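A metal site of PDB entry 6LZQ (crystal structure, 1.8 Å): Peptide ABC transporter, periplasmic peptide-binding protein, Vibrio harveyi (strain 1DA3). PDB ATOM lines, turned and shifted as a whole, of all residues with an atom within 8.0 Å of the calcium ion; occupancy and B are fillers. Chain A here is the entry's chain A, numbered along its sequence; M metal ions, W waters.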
ATOM      1  N   LYS A 339      -9.848 -32.492 -20.704  1.00  0.00           N
ATOM      2  CA  LYS A 339     -10.315 -32.495 -19.327  1.00  0.00           C
ATOM      3  C   LYS A 339     -10.043 -31.142 -18.672  1.00  0.00           C
ATOM      4  O   LYS A 339      -8.987 -30.563 -18.878  1.00  0.00           O
ATOM      5  CB  LYS A 339      -9.625 -33.622 -18.585  1.00  0.00           C
ATOM      6  CG  LYS A 339      -9.922 -33.706 -17.103  1.00  0.00           C
ATOM      7  CD  LYS A 339      -8.992 -34.759 -16.490  1.00  0.00           C
ATOM      8  CE  LYS A 339      -9.063 -34.713 -14.987  1.00  0.00           C
ATOM      9  NZ  LYS A 339     -10.456 -34.844 -14.542  1.00  0.00           N
ATOM     10  N   ASP A 340     -10.995 -30.630 -17.896  1.00  0.00           N
ATOM     11  CA  ASP A 340     -10.758 -29.394 -17.149  1.00  0.00           C
ATOM     12  C   ASP A 340      -9.840 -29.703 -15.974  1.00  0.00           C
ATOM     13  O   ASP A 340     -10.252 -30.417 -15.050  1.00  0.00           O
ATOM     14  CB  ASP A 340     -12.074 -28.792 -16.652  1.00  0.00           C
ATOM     15  CG  ASP A 340     -11.879 -27.516 -15.833  1.00  0.00           C
ATOM     16  OD1 ASP A 340     -10.826 -26.846 -15.985  1.00  0.00           O
ATOM     17  OD2 ASP A 340     -12.776 -27.187 -15.036  1.00  0.00           O
ATOM     18  N   VAL A 341      -8.622 -29.185 -15.982  1.00  0.00           N
ATOM     19  CA  VAL A 341      -7.705 -29.497 -14.888  1.00  0.00           C
ATOM     20  C   VAL A 341      -7.343 -28.271 -14.059  1.00  0.00           C
ATOM     21  O   VAL A 341      -6.450 -28.339 -13.204  1.00  0.00           O
ATOM     22  CB  VAL A 341      -6.425 -30.196 -15.391  1.00  0.00           C
ATOM     23  CG1 VAL A 341      -6.763 -31.613 -15.897  1.00  0.00           C
ATOM     24  CG2 VAL A 341      -5.713 -29.395 -16.472  1.00  0.00           C
ATOM     25  N   ASN A 342      -8.043 -27.160 -14.264  1.00  0.00           N
ATOM     26  CA  ASN A 342      -7.827 -26.009 -13.379  1.00  0.00           C
ATOM     27  C   ASN A 342      -9.115 -25.351 -12.882  1.00  0.00           C
ATOM     28  O   ASN A 342      -9.136 -24.150 -12.622  1.00  0.00           O
ATOM     29  CB  ASN A 342      -6.904 -24.979 -14.037  1.00  0.00           C
ATOM     30  CG  ASN A 342      -7.541 -24.304 -15.240  1.00  0.00           C
ATOM     31  OD1 ASN A 342      -8.613 -24.693 -15.678  1.00  0.00           O
ATOM     32  ND2 ASN A 342      -6.875 -23.289 -15.763  1.00  0.00           N
ATOM     33  N   LYS A 343     -10.164 -26.142 -12.740  1.00  0.00           N
ATOM     34  CA  LYS A 343     -11.375 -25.751 -12.009  1.00  0.00           C
ATOM     35  C   LYS A 343     -12.047 -24.479 -12.507  1.00  0.00           C
ATOM     36  O   LYS A 343     -12.629 -23.753 -11.713  1.00  0.00           O
ATOM     37  CB  LYS A 343     -11.058 -25.575 -10.514  1.00  0.00           C
ATOM     38  CG  LYS A 343     -10.303 -26.745  -9.906  1.00  0.00           C
ATOM     39  CD  LYS A 343     -10.239 -26.639  -8.395  1.00  0.00           C
ATOM     40  CE  LYS A 343      -9.404 -27.759  -7.825  1.00  0.00           C
ATOM     41  NZ  LYS A 343      -8.044 -27.777  -8.462  1.00  0.00           N
ATOM     42  N   ASP A 344     -11.993 -24.208 -13.815  1.00  0.00           N
ATOM     43  CA  ASP A 344     -12.680 -23.021 -14.313  1.00  0.00           C
ATOM     44  C   ASP A 344     -13.859 -23.421 -15.204  1.00  0.00           C
ATOM     45  O   ASP A 344     -14.523 -22.562 -15.792  1.00  0.00           O
ATOM     46  CB  ASP A 344     -11.701 -22.081 -15.049  1.00  0.00           C
ATOM     47  CG  ASP A 344     -11.232 -22.631 -16.396  1.00  0.00           C
ATOM     48  OD1 ASP A 344     -11.345 -23.843 -16.646  1.00  0.00           O
ATOM     49  OD2 ASP A 344     -10.724 -21.813 -17.211  1.00  0.00           O
ATOM     50  N   GLY A 345     -14.142 -24.715 -15.286  1.00  0.00           N
ATOM     51  CA  GLY A 345     -15.273 -25.195 -16.061  1.00  0.00           C
ATOM     52  C   GLY A 345     -15.010 -25.299 -17.553  1.00  0.00           C
ATOM     53  O   GLY A 345     -15.887 -25.694 -18.312  1.00  0.00           O
ATOM     54  N   PHE A 346     -13.814 -24.931 -17.981  1.00  0.00           N
ATOM     55  CA  PHE A 346     -13.478 -24.998 -19.403  1.00  0.00           C
ATOM     56  C   PHE A 346     -12.424 -26.073 -19.657  1.00  0.00           C
ATOM     57  O   PHE A 346     -11.428 -26.158 -18.936  1.00  0.00           O
ATOM     58  CB  PHE A 346     -13.006 -23.632 -19.910  1.00  0.00           C
ATOM     59  CG  PHE A 346     -14.092 -22.586 -19.926  1.00  0.00           C
ATOM     60  CD1 PHE A 346     -15.124 -22.679 -20.851  1.00  0.00           C
ATOM     61  CD2 PHE A 346     -14.094 -21.542 -19.023  1.00  0.00           C
ATOM     62  CE1 PHE A 346     -16.143 -21.735 -20.876  1.00  0.00           C
ATOM     63  CE2 PHE A 346     -15.105 -20.592 -19.026  1.00  0.00           C
ATOM     64  CZ  PHE A 346     -16.131 -20.682 -19.958  1.00  0.00           C
ATOM     65  N   VAL A 347     -12.637 -26.904 -20.684  1.00  0.00           N
ATOM     66  CA  VAL A 347     -11.743 -28.032 -20.896  1.00  0.00           C
ATOM     67  C   VAL A 347     -10.373 -27.520 -21.298  1.00  0.00           C
ATOM     68  O   VAL A 347     -10.242 -26.470 -21.912  1.00  0.00           O
ATOM     69  CB  VAL A 347     -12.257 -29.004 -21.994  1.00  0.00           C
ATOM     70  CG1 VAL A 347     -13.653 -29.519 -21.639  1.00  0.00           C
ATOM     71  CG2 VAL A 347     -12.234 -28.355 -23.399  1.00  0.00           C
ATOM     72  N   ASP A 348      -9.352 -28.274 -20.909  1.00  0.00           N
ATOM     73  CA  ASP A 348      -7.996 -27.967 -21.285  1.00  0.00           C
ATOM     74  C   ASP A 348      -7.516 -29.046 -22.235  1.00  0.00           C
ATOM     75  O   ASP A 348      -8.162 -30.086 -22.345  1.00  0.00           O
ATOM     76  CB  ASP A 348      -7.133 -27.847 -20.025  1.00  0.00           C
ATOM     77  CG  ASP A 348      -7.765 -26.887 -19.010  1.00  0.00           C
ATOM     78  OD1 ASP A 348      -7.932 -25.705 -19.380  1.00  0.00           O
ATOM     79  OD2 ASP A 348      -8.127 -27.288 -17.880  1.00  0.00           O
ATOM     80  N   THR A 349      -6.399 -28.808 -22.924  1.00  0.00           N
ATOM     81  CA  THR A 349      -5.923 -29.792 -23.884  1.00  0.00           C
ATOM     82  C   THR A 349      -5.459 -31.073 -23.198  1.00  0.00           C
ATOM     83  O   THR A 349      -5.248 -31.090 -21.980  1.00  0.00           O
ATOM     84  CB  THR A 349      -4.749 -29.250 -24.704  1.00  0.00           C
ATOM     85  OG1 THR A 349      -3.594 -29.164 -23.856  1.00  0.00           O
ATOM     86  CG2 THR A 349      -5.096 -27.887 -25.311  1.00  0.00           C
ATOM     87  N   GLY A 352      -2.696 -30.615 -20.952  1.00  0.00           N
ATOM     88  CA  GLY A 352      -3.056 -29.906 -19.742  1.00  0.00           C
ATOM     89  C   GLY A 352      -3.105 -28.399 -19.862  1.00  0.00           C
ATOM     90  O   GLY A 352      -3.221 -27.684 -18.854  1.00  0.00           O
ATOM     91  N   LYS A 353      -3.029 -27.905 -21.093  1.00  0.00           N
ATOM     92  CA  LYS A 353      -2.929 -26.458 -21.312  1.00  0.00           C
ATOM     93  C   LYS A 353      -4.275 -25.810 -21.478  1.00  0.00           C
ATOM     94  O   LYS A 353      -5.134 -26.325 -22.198  1.00  0.00           O
ATOM     95  CB  LYS A 353      -2.100 -26.162 -22.559  1.00  0.00           C
ATOM     96  CG  LYS A 353      -0.713 -26.721 -22.541  1.00  0.00           C
ATOM     97  CD  LYS A 353      -0.053 -26.528 -23.901  1.00  0.00           C
ATOM     98  CE  LYS A 353       1.294 -27.226 -23.934  1.00  0.00           C
ATOM     99  NZ  LYS A 353       2.076 -26.904 -22.710  1.00  0.00           N
ATOM    100  N   SER A 354      -4.443 -24.648 -20.848  1.00  0.00           N
ATOM    101  CA  SER A 354      -5.660 -23.867 -21.014  1.00  0.00           C
ATOM    102  C   SER A 354      -5.606 -23.121 -22.324  1.00  0.00           C
ATOM    103  O   SER A 354      -4.527 -22.852 -22.849  1.00  0.00           O
ATOM    104  CB  SER A 354      -5.855 -22.884 -19.862  1.00  0.00           C
ATOM    105  OG  SER A 354      -6.243 -23.576 -18.690  1.00  0.00           O
ATOM    106  N   PHE A 355      -6.772 -22.809 -22.866  1.00  0.00           N
ATOM    107  CA  PHE A 355      -6.837 -22.092 -24.121  1.00  0.00           C
ATOM    108  C   PHE A 355      -8.207 -21.477 -24.290  1.00  0.00           C
ATOM    109  O   PHE A 355      -9.192 -21.953 -23.747  1.00  0.00           O
ATOM    110  CB  PHE A 355      -6.505 -23.008 -25.301  1.00  0.00           C
ATOM    111  CG  PHE A 355      -7.519 -24.083 -25.541  1.00  0.00           C
ATOM    112  CD1 PHE A 355      -7.485 -25.268 -24.817  1.00  0.00           C
ATOM    113  CD2 PHE A 355      -8.527 -23.909 -26.489  1.00  0.00           C
ATOM    114  CE1 PHE A 355      -8.424 -26.265 -25.037  1.00  0.00           C
ATOM    115  CE2 PHE A 355      -9.481 -24.898 -26.706  1.00  0.00           C
ATOM    116  CZ  PHE A 355      -9.427 -26.071 -25.976  1.00  0.00           C
ATOM    117  N   GLY A 383     -18.332 -26.468 -22.274  1.00  0.00           N
ATOM    118  CA  GLY A 383     -17.025 -26.280 -21.654  1.00  0.00           C
ATOM    119  C   GLY A 383     -15.903 -25.895 -22.592  1.00  0.00           C
ATOM    120  O   GLY A 383     -14.738 -26.038 -22.256  1.00  0.00           O
ATOM    121  N   LYS A 385     -14.002 -22.873 -24.216  1.00  0.00           N
ATOM    122  CA  LYS A 385     -13.849 -21.432 -24.043  1.00  0.00           C
ATOM    123  C   LYS A 385     -13.518 -20.749 -25.354  1.00  0.00           C
ATOM    124  O   LYS A 385     -12.567 -21.121 -26.059  1.00  0.00           O
ATOM    125  CB  LYS A 385     -12.765 -21.141 -23.000  1.00  0.00           C
ATOM    126  CG  LYS A 385     -12.868 -19.770 -22.382  1.00  0.00           C
ATOM    127  CD  LYS A 385     -11.778 -19.610 -21.350  1.00  0.00           C
ATOM    128  CE  LYS A 385     -11.858 -18.269 -20.632  1.00  0.00           C
ATOM    129  NZ  LYS A 385     -10.621 -18.050 -19.821  1.00  0.00           N
HETATM  130 CA    CA M   1      -9.783 -25.408 -17.542  1.00  0.00          CA
HETATM  131  O   HOH W   1      -9.354 -23.299 -18.740  1.00  0.00           O
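The calcium ion is bound by the backbone carbonyl oxygen (O) of Phe 346, the side-chain amide oxygen (OD1) of Asn 342, the side-chain carboxylate (OD1) of Asp 340, the side-chain carboxylate (OD1) of Asp 344, water W1, the side-chain carboxylate (OD2) of Asp 348 and the side-chain carboxylate (OD1) of Asp 348.
The calcium ion has seven donor atoms within binding distance.
Water W1 bridges OD2 of Asp 344 (2.5 Å) and OG of Ser 354 (3.1 Å).
OD2 of Asp 348 lies close to N of Val 341 (2.7 Å).
The side-chain carboxylate of Asp 340 sits close to the backbone NH of Lys 343 (3.4 Å).
OD2 of Asp 340 lies within hydrogen-bond range of N of Gly 345, 2.8 Å away.
ND2 of Asn 342 is in hydrogen-bond range of OG of Ser 354 (3.0 Å).
The side-chain carboxylate (OD1) of Asp 348 lies close to the side-chain hydroxyl (OG) of Ser 354.
The backbone NH of Asp 348 lies within hydrogen-bond range of the backbone carbonyl oxygen of Lys 339.
Within 4 Å of the calcium ion: Asp 340, Asn 342, Asp 344, Phe 346 and Asp 348.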
